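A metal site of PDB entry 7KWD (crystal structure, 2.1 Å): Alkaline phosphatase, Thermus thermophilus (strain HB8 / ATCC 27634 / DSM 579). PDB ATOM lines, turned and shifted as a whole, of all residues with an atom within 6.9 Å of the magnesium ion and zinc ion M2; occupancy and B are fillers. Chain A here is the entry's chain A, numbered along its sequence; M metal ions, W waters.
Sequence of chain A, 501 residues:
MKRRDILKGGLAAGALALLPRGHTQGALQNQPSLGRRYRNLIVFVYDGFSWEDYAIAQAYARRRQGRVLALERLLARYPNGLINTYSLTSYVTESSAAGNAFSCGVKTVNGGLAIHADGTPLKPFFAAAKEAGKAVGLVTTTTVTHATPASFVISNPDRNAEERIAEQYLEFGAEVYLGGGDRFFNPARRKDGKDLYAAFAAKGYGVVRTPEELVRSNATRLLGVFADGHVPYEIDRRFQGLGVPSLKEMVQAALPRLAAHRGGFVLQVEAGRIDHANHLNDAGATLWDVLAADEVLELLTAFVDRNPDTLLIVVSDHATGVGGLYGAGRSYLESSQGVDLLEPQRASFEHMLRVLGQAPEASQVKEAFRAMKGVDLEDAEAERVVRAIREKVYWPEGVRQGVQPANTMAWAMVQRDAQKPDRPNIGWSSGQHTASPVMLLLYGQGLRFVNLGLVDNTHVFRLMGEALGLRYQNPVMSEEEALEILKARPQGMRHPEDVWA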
ATOM      1  N   VAL A  45      -2.486   7.451 -12.218  1.00  0.00           N
ATOM      2  CA  VAL A  45      -1.705   6.797 -11.158  1.00  0.00           C
ATOM      3  C   VAL A  45      -0.950   5.619 -11.758  1.00  0.00           C
ATOM      4  O   VAL A  45      -1.557   4.719 -12.353  1.00  0.00           O
ATOM      5  CB  VAL A  45      -2.593   6.323 -10.011  1.00  0.00           C
ATOM      6  CG1 VAL A  45      -1.740   5.628  -8.950  1.00  0.00           C
ATOM      7  CG2 VAL A  45      -3.381   7.486  -9.448  1.00  0.00           C
ATOM      8  N   TYR A  46       0.365   5.614 -11.582  1.00  0.00           N
ATOM      9  CA  TYR A  46       1.222   4.454 -11.820  1.00  0.00           C
ATOM     10  C   TYR A  46       1.375   3.728 -10.491  1.00  0.00           C
ATOM     11  O   TYR A  46       2.173   4.108  -9.643  1.00  0.00           O
ATOM     12  CB  TYR A  46       2.572   4.903 -12.357  1.00  0.00           C
ATOM     13  CG  TYR A  46       2.678   5.271 -13.828  1.00  0.00           C
ATOM     14  CD1 TYR A  46       1.929   6.298 -14.380  1.00  0.00           C
ATOM     15  CD2 TYR A  46       3.622   4.652 -14.649  1.00  0.00           C
ATOM     16  CE1 TYR A  46       2.079   6.658 -15.710  1.00  0.00           C
ATOM     17  CE2 TYR A  46       3.784   5.009 -15.972  1.00  0.00           C
ATOM     18  CZ  TYR A  46       3.013   6.013 -16.495  1.00  0.00           C
ATOM     19  OH  TYR A  46       3.148   6.355 -17.820  1.00  0.00           O
ATOM     20  N   ASP A  47       0.587   2.673 -10.266  1.00  0.00           N
ATOM     21  CA  ASP A  47       0.595   2.006  -8.977  1.00  0.00           C
ATOM     22  C   ASP A  47       1.853   1.169  -8.814  1.00  0.00           C
ATOM     23  O   ASP A  47       2.168   0.338  -9.657  1.00  0.00           O
ATOM     24  CB  ASP A  47      -0.652   1.130  -8.828  1.00  0.00           C
ATOM     25  CG  ASP A  47      -0.950   0.844  -7.404  1.00  0.00           C
ATOM     26  OD1 ASP A  47      -0.032   0.317  -6.747  1.00  0.00           O
ATOM     27  OD2 ASP A  47      -2.075   1.169  -6.932  1.00  0.00           O
ATOM     28  N   GLY A  48       2.572   1.387  -7.715  1.00  0.00           N
ATOM     29  CA  GLY A  48       3.757   0.592  -7.415  1.00  0.00           C
ATOM     30  C   GLY A  48       4.994   0.903  -8.232  1.00  0.00           C
ATOM     31  O   GLY A  48       5.977   0.145  -8.180  1.00  0.00           O
ATOM     32  N   THR A  93       3.598   2.456   2.943  1.00  0.00           N
ATOM     33  CA  THR A  93       2.149   2.539   2.823  1.00  0.00           C
ATOM     34  C   THR A  93       1.655   1.337   2.031  1.00  0.00           C
ATOM     35  O   THR A  93       2.406   0.656   1.352  1.00  0.00           O
ATOM     36  CB  THR A  93       1.769   3.824   2.093  1.00  0.00           C
ATOM     37  OG1 THR A  93       0.367   4.084   2.150  1.00  0.00           O
ATOM     38  CG2 THR A  93       2.175   3.716   0.636  1.00  0.00           C
ATOM     39  N   GLU A  94       0.350   1.122   2.066  1.00  0.00           N
ATOM     40  CA  GLU A  94      -0.256   0.375   0.954  1.00  0.00           C
ATOM     41  C   GLU A  94      -1.253   1.295   0.247  1.00  0.00           C
ATOM     42  O   GLU A  94      -1.329   2.501   0.509  1.00  0.00           O
ATOM     43  CB  GLU A  94      -0.839  -0.961   1.425  1.00  0.00           C
ATOM     44  CG  GLU A  94      -1.691  -0.870   2.649  1.00  0.00           C
ATOM     45  CD  GLU A  94      -2.940  -0.013   2.372  1.00  0.00           C
ATOM     46  OE1 GLU A  94      -2.887   1.203   2.677  1.00  0.00           O
ATOM     47  OE2 GLU A  94      -3.956  -0.542   1.839  1.00  0.00           O
ATOM     48  N   SER A  95      -2.021   0.696  -0.668  1.00  0.00           N
ATOM     49  CA  SER A  95      -2.690   1.475  -1.693  1.00  0.00           C
ATOM     50  C   SER A  95      -3.841   2.318  -1.143  1.00  0.00           C
ATOM     51  O   SER A  95      -4.093   3.424  -1.647  1.00  0.00           O
ATOM     52  CB  SER A  95      -3.200   0.550  -2.779  1.00  0.00           C
ATOM     53  OG  SER A  95      -2.286   0.449  -3.818  1.00  0.00           O
ATOM     54  N   SER A  96      -4.590   1.818  -0.143  1.00  0.00           N
ATOM     55  CA  SER A  96      -5.734   2.593   0.348  1.00  0.00           C
ATOM     56  C   SER A  96      -5.274   3.850   1.074  1.00  0.00           C
ATOM     57  O   SER A  96      -5.795   4.946   0.832  1.00  0.00           O
ATOM     58  CB  SER A  96      -6.636   1.767   1.278  1.00  0.00           C
ATOM     59  OG  SER A  96      -5.895   1.189   2.327  1.00  0.00           O
ATOM     60  N   ALA A  98      -2.439   5.320   0.609  1.00  0.00           N
ATOM     61  CA  ALA A  98      -1.818   6.195  -0.389  1.00  0.00           C
ATOM     62  C   ALA A  98      -2.886   6.919  -1.180  1.00  0.00           C
ATOM     63  O   ALA A  98      -2.824   8.142  -1.356  1.00  0.00           O
ATOM     64  CB  ALA A  98      -0.934   5.366  -1.306  1.00  0.00           C
ATOM     65  N   THR A 140      -9.284   1.491 -14.879  1.00  0.00           N
ATOM     66  CA  THR A 140      -8.118   0.829 -14.300  1.00  0.00           C
ATOM     67  C   THR A 140      -7.936  -0.577 -14.851  1.00  0.00           C
ATOM     68  O   THR A 140      -8.861  -1.154 -15.406  1.00  0.00           O
ATOM     69  CB  THR A 140      -8.252   0.744 -12.781  1.00  0.00           C
ATOM     70  OG1 THR A 140      -7.171  -0.010 -12.225  1.00  0.00           O
ATOM     71  CG2 THR A 140      -9.574   0.075 -12.398  1.00  0.00           C
ATOM     72  N   THR A 142      -6.842  -2.868 -12.605  1.00  0.00           N
ATOM     73  CA  THR A 142      -7.267  -3.709 -11.497  1.00  0.00           C
ATOM     74  C   THR A 142      -8.772  -3.947 -11.589  1.00  0.00           C
ATOM     75  O   THR A 142      -9.458  -3.398 -12.464  1.00  0.00           O
ATOM     76  CB  THR A 142      -6.911  -3.069 -10.156  1.00  0.00           C
ATOM     77  OG1 THR A 142      -7.685  -1.870  -9.993  1.00  0.00           O
ATOM     78  CG2 THR A 142      -5.411  -2.721 -10.064  1.00  0.00           C
ATOM     79  N   HIS A 146     -11.185  -1.736  -6.855  1.00  0.00           N
ATOM     80  CA  HIS A 146      -9.959  -1.814  -6.082  1.00  0.00           C
ATOM     81  C   HIS A 146      -9.649  -0.480  -5.407  1.00  0.00           C
ATOM     82  O   HIS A 146     -10.330   0.530  -5.608  1.00  0.00           O
ATOM     83  CB  HIS A 146      -8.825  -2.279  -6.983  1.00  0.00           C
ATOM     84  CG  HIS A 146      -7.774  -3.084  -6.291  1.00  0.00           C
ATOM     85  ND1 HIS A 146      -6.457  -2.698  -6.253  1.00  0.00           N
ATOM     86  CD2 HIS A 146      -7.843  -4.287  -5.654  1.00  0.00           C
ATOM     87  CE1 HIS A 146      -5.753  -3.609  -5.611  1.00  0.00           C
ATOM     88  NE2 HIS A 146      -6.567  -4.583  -5.226  1.00  0.00           N
ATOM     89  N   ALA A 147      -8.630  -0.508  -4.550  1.00  0.00           N
ATOM     90  CA  ALA A 147      -8.425   0.575  -3.588  1.00  0.00           C
ATOM     91  C   ALA A 147      -8.175   1.906  -4.270  1.00  0.00           C
ATOM     92  O   ALA A 147      -8.701   2.937  -3.824  1.00  0.00           O
ATOM     93  CB  ALA A 147      -7.246   0.249  -2.680  1.00  0.00           C
ATOM     94  N   THR A 148      -7.398   1.924  -5.349  1.00  0.00           N
ATOM     95  CA  THR A 148      -6.970   3.218  -5.875  1.00  0.00           C
ATOM     96  C   THR A 148      -8.132   3.980  -6.475  1.00  0.00           C
ATOM     97  O   THR A 148      -8.339   5.147  -6.111  1.00  0.00           O
ATOM     98  CB  THR A 148      -5.839   3.008  -6.879  1.00  0.00           C
ATOM     99  OG1 THR A 148      -4.716   2.409  -6.220  1.00  0.00           O
ATOM    100  CG2 THR A 148      -5.438   4.337  -7.460  1.00  0.00           C
ATOM    101  N   PRO A 149      -8.942   3.405  -7.361  1.00  0.00           N
ATOM    102  CA  PRO A 149     -10.145   4.124  -7.818  1.00  0.00           C
ATOM    103  C   PRO A 149     -11.127   4.347  -6.702  1.00  0.00           C
ATOM    104  O   PRO A 149     -11.719   5.444  -6.588  1.00  0.00           O
ATOM    105  CB  PRO A 149     -10.717   3.196  -8.911  1.00  0.00           C
ATOM    106  CG  PRO A 149     -10.064   1.869  -8.701  1.00  0.00           C
ATOM    107  CD  PRO A 149      -8.701   2.159  -8.097  1.00  0.00           C
ATOM    108  N   ARG A 159     -11.055  -2.164   2.569  1.00  0.00           N
ATOM    109  CA  ARG A 159     -10.799  -2.053   1.141  1.00  0.00           C
ATOM    110  C   ARG A 159     -11.195  -3.323   0.412  1.00  0.00           C
ATOM    111  O   ARG A 159     -11.549  -3.282  -0.764  1.00  0.00           O
ATOM    112  CB  ARG A 159      -9.316  -1.737   0.871  1.00  0.00           C
ATOM    113  CG  ARG A 159      -8.302  -2.719   1.459  1.00  0.00           C
ATOM    114  CD  ARG A 159      -6.876  -2.489   0.952  1.00  0.00           C
ATOM    115  NE  ARG A 159      -6.702  -2.707  -0.495  1.00  0.00           N
ATOM    116  CZ  ARG A 159      -5.553  -2.537  -1.142  1.00  0.00           C
ATOM    117  NH1 ARG A 159      -5.452  -2.793  -2.443  1.00  0.00           N
ATOM    118  NH2 ARG A 159      -4.479  -2.116  -0.462  1.00  0.00           N
ATOM    119  N   GLN A 268      -9.791   9.410 -13.155  1.00  0.00           N
ATOM    120  CA  GLN A 268      -8.636   8.680 -12.691  1.00  0.00           C
ATOM    121  C   GLN A 268      -8.359   7.552 -13.694  1.00  0.00           C
ATOM    122  O   GLN A 268      -9.272   6.786 -14.045  1.00  0.00           O
ATOM    123  CB  GLN A 268      -8.826   8.093 -11.289  1.00  0.00           C
ATOM    124  CG  GLN A 268      -7.536   7.458 -10.743  1.00  0.00           C
ATOM    125  CD  GLN A 268      -7.734   6.552  -9.536  1.00  0.00           C
ATOM    126  OE1 GLN A 268      -7.790   5.339  -9.653  1.00  0.00           O
ATOM    127  NE2 GLN A 268      -7.766   7.154  -8.350  1.00  0.00           N
ATOM    128  N   GLU A 270      -5.742   4.367 -13.927  1.00  0.00           N
ATOM    129  CA  GLU A 270      -4.799   3.625 -13.097  1.00  0.00           C
ATOM    130  C   GLU A 270      -4.107   2.536 -13.905  1.00  0.00           C
ATOM    131  O   GLU A 270      -4.773   1.649 -14.460  1.00  0.00           O
ATOM    132  CB  GLU A 270      -5.450   2.982 -11.876  1.00  0.00           C
ATOM    133  CG  GLU A 270      -4.340   2.640 -10.834  1.00  0.00           C
ATOM    134  CD  GLU A 270      -4.767   1.577  -9.883  1.00  0.00           C
ATOM    135  OE1 GLU A 270      -5.885   1.039 -10.070  1.00  0.00           O
ATOM    136  OE2 GLU A 270      -3.994   1.312  -8.959  1.00  0.00           O
ATOM    137  N   ALA A 271      -2.786   2.615 -13.972  1.00  0.00           N
ATOM    138  CA  ALA A 271      -1.959   1.501 -14.404  1.00  0.00           C
ATOM    139  C   ALA A 271      -1.668   0.726 -13.137  1.00  0.00           C
ATOM    140  O   ALA A 271      -0.615   0.843 -12.517  1.00  0.00           O
ATOM    141  CB  ALA A 271      -0.690   1.976 -15.097  1.00  0.00           C
ATOM    142  N   GLY A 272      -2.677  -0.063 -12.719  1.00  0.00           N
ATOM    143  CA  GLY A 272      -2.668  -0.619 -11.395  1.00  0.00           C
ATOM    144  C   GLY A 272      -1.917  -1.898 -11.220  1.00  0.00           C
ATOM    145  O   GLY A 272      -1.779  -2.372 -10.079  1.00  0.00           O
ATOM    146  N   ARG A 273      -1.430  -2.512 -12.306  1.00  0.00           N
ATOM    147  CA  ARG A 273      -0.785  -3.811 -12.174  1.00  0.00           C
ATOM    148  C   ARG A 273       0.721  -3.735 -12.325  1.00  0.00           C
ATOM    149  O   ARG A 273       1.412  -4.768 -12.229  1.00  0.00           O
ATOM    150  CB  ARG A 273      -1.393  -4.800 -13.185  1.00  0.00           C
ATOM    151  CG  ARG A 273      -2.934  -4.883 -13.066  1.00  0.00           C
ATOM    152  CD  ARG A 273      -3.534  -6.262 -13.397  1.00  0.00           C
ATOM    153  NE  ARG A 273      -3.131  -7.246 -12.389  1.00  0.00           N
ATOM    154  CZ  ARG A 273      -3.086  -8.554 -12.599  1.00  0.00           C
ATOM    155  NH1 ARG A 273      -3.427  -9.059 -13.781  1.00  0.00           N
ATOM    156  NH2 ARG A 273      -2.691  -9.338 -11.617  1.00  0.00           N
ATOM    157  N   ASP A 275       2.293  -2.399  -9.895  1.00  0.00           N
ATOM    158  CA  ASP A 275       2.441  -2.897  -8.525  1.00  0.00           C
ATOM    159  C   ASP A 275       2.427  -4.413  -8.483  1.00  0.00           C
ATOM    160  O   ASP A 275       3.342  -5.043  -7.942  1.00  0.00           O
ATOM    161  CB  ASP A 275       1.312  -2.305  -7.665  1.00  0.00           C
ATOM    162  CG  ASP A 275       1.393  -2.689  -6.224  1.00  0.00           C
ATOM    163  OD1 ASP A 275       2.428  -2.352  -5.588  1.00  0.00           O
ATOM    164  OD2 ASP A 275       0.418  -3.307  -5.728  1.00  0.00           O
ATOM    165  N   HIS A 276       1.429  -5.035  -9.108  1.00  0.00           N
ATOM    166  CA  HIS A 276       1.270  -6.477  -9.023  1.00  0.00           C
ATOM    167  C   HIS A 276       2.460  -7.207  -9.622  1.00  0.00           C
ATOM    168  O   HIS A 276       2.968  -8.168  -9.051  1.00  0.00           O
ATOM    169  CB  HIS A 276      -0.013  -6.915  -9.735  1.00  0.00           C
ATOM    170  CG  HIS A 276      -1.240  -6.324  -9.118  1.00  0.00           C
ATOM    171  ND1 HIS A 276      -2.480  -6.451  -9.689  1.00  0.00           N
ATOM    172  CD2 HIS A 276      -1.421  -5.581  -8.003  1.00  0.00           C
ATOM    173  CE1 HIS A 276      -3.383  -5.835  -8.944  1.00  0.00           C
ATOM    174  NE2 HIS A 276      -2.763  -5.293  -7.922  1.00  0.00           N
ATOM    175  N   ASP A 317       1.879   6.008  -6.677  1.00  0.00           N
ATOM    176  CA  ASP A 317       1.389   6.030  -5.289  1.00  0.00           C
ATOM    177  C   ASP A 317       2.384   5.497  -4.275  1.00  0.00           C
ATOM    178  O   ASP A 317       2.255   5.800  -3.083  1.00  0.00           O
ATOM    179  CB  ASP A 317       0.052   5.304  -5.161  1.00  0.00           C
ATOM    180  CG  ASP A 317       0.149   3.826  -5.363  1.00  0.00           C
ATOM    181  OD1 ASP A 317       1.086   3.327  -6.041  1.00  0.00           O
ATOM    182  OD2 ASP A 317      -0.756   3.138  -4.860  1.00  0.00           O
ATOM    183  N   HIS A 318       3.363   4.711  -4.710  1.00  0.00           N
ATOM    184  CA  HIS A 318       4.478   4.239  -3.904  1.00  0.00           C
ATOM    185  C   HIS A 318       5.311   3.324  -4.812  1.00  0.00           C
ATOM    186  O   HIS A 318       4.837   2.853  -5.856  1.00  0.00           O
ATOM    187  CB  HIS A 318       4.044   3.432  -2.671  1.00  0.00           C
ATOM    188  CG  HIS A 318       3.124   2.326  -3.046  1.00  0.00           C
ATOM    189  ND1 HIS A 318       3.568   1.139  -3.583  1.00  0.00           N
ATOM    190  CD2 HIS A 318       1.781   2.275  -3.077  1.00  0.00           C
ATOM    191  CE1 HIS A 318       2.535   0.386  -3.887  1.00  0.00           C
ATOM    192  NE2 HIS A 318       1.442   1.047  -3.574  1.00  0.00           N
ATOM    193  N   THR A 320       7.346  -0.328  -5.361  1.00  0.00           N
ATOM    194  CA  THR A 320       7.166  -1.727  -5.006  1.00  0.00           C
ATOM    195  C   THR A 320       8.294  -2.572  -5.575  1.00  0.00           C
ATOM    196  O   THR A 320       8.644  -2.438  -6.756  1.00  0.00           O
ATOM    197  CB  THR A 320       5.815  -2.252  -5.483  1.00  0.00           C
ATOM    198  OG1 THR A 320       4.810  -1.489  -4.845  1.00  0.00           O
ATOM    199  CG2 THR A 320       5.627  -3.751  -5.129  1.00  0.00           C
ATOM    200  N   HIS A 433       5.865  -3.449  -1.044  1.00  0.00           N
ATOM    201  CA  HIS A 433       6.106  -2.017  -1.224  1.00  0.00           C
ATOM    202  C   HIS A 433       7.360  -1.575  -0.487  1.00  0.00           C
ATOM    203  O   HIS A 433       7.790  -2.202   0.489  1.00  0.00           O
ATOM    204  CB  HIS A 433       4.951  -1.171  -0.695  1.00  0.00           C
ATOM    205  CG  HIS A 433       3.637  -1.552  -1.250  1.00  0.00           C
ATOM    206  ND1 HIS A 433       2.455  -1.003  -0.810  1.00  0.00           N
ATOM    207  CD2 HIS A 433       3.294  -2.450  -2.220  1.00  0.00           C
ATOM    208  CE1 HIS A 433       1.441  -1.540  -1.473  1.00  0.00           C
ATOM    209  NE2 HIS A 433       1.924  -2.423  -2.315  1.00  0.00           N
HETATM  210 MG    MG M   1      -4.046   0.339  -7.174  1.00  0.00          MG
HETATM  211 ZN    ZN M   2      -0.498   0.982  -4.694  1.00  0.00          ZN
HETATM  212 ZN    ZN M   3       0.850  -3.597  -3.813  1.00  0.00          ZN
HETATM  213  O   HOH W   1      -2.983  -1.592  -7.921  1.00  0.00           O
HETATM  214  O   HOH W   2      -4.211  -0.539  -5.440  1.00  0.00           O
HETATM  215  O   HOH W   3      -6.119  -0.082  -7.387  1.00  0.00           O
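The magnesium ion is bound by water W2 (2.0 Å), the side-chain carboxylate of Glu 270 (2.0 Å), water W3 (2.1 Å), the side-chain carboxylate of Asp 47 (2.2 Å), water W1 (2.3 Å) and the side-chain hydroxyl of Thr 148 (2.4 Å). The magnesium ion has six donor atoms within binding distance.
A ring nitrogen (NE2) of His 146 sits close to the guanidinium group of Arg 159, at 3.5 Å. OG1 of Thr 140 is in hydrogen-bond range of OE1 of Glu 270. OE1 of Glu 270 lies within hydrogen-bond range of OG1 of Thr 142. NE2 of Gln 268 sits at hydrogen-bond distance from O of Thr 148 (3.1 Å). The backbone NH (N) of Asp 275 is in hydrogen-bond range of the backbone carbonyl oxygen (O) of Asp 47 (2.8 Å). The backbone NH (N) of Asp 47 is in hydrogen-bond range of the backbone carbonyl oxygen (O) of Ala 271, at 3.1 Å. The backbone carbonyl oxygen of His 318 lies close to the backbone NH of Gly 48 (3.3 Å). The side-chain carboxylate (OD1) of Asp 317 lies within hydrogen-bond range of the backbone NH (N) of Gly 48 (3.0 Å).
Water W3 lies within hydrogen-bond range of a ring nitrogen (ND1) of His 146, the side-chain carboxylate of Glu 270 and the backbone NH of Thr 148.
Along chain A the residues within 4 Å of zinc ion M2 span positions 47 to 318. The nearest printed residue that does not touch zinc ion M2 is Gly 48 (4.3 Å).
His 146 touches the magnesium ion (ND1 to MG, 3.99 Å). Of the 27 residues printed, 5 come within 4 Å of the magnesium ion. The nearest printed residue that does not touch the magnesium ion is Thr 142 (4.4 Å).
Zinc ion M2 is bound by OG of Ser 95, OD2 of Asp 317, OD1 of Asp 47 and NE2 of His 318. Zinc ion M2 has four donor atoms within binding distance. Slightly farther from zinc ion M2 lies the side-chain carboxylate (OD2) of Asp 47 (2.7 Å).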
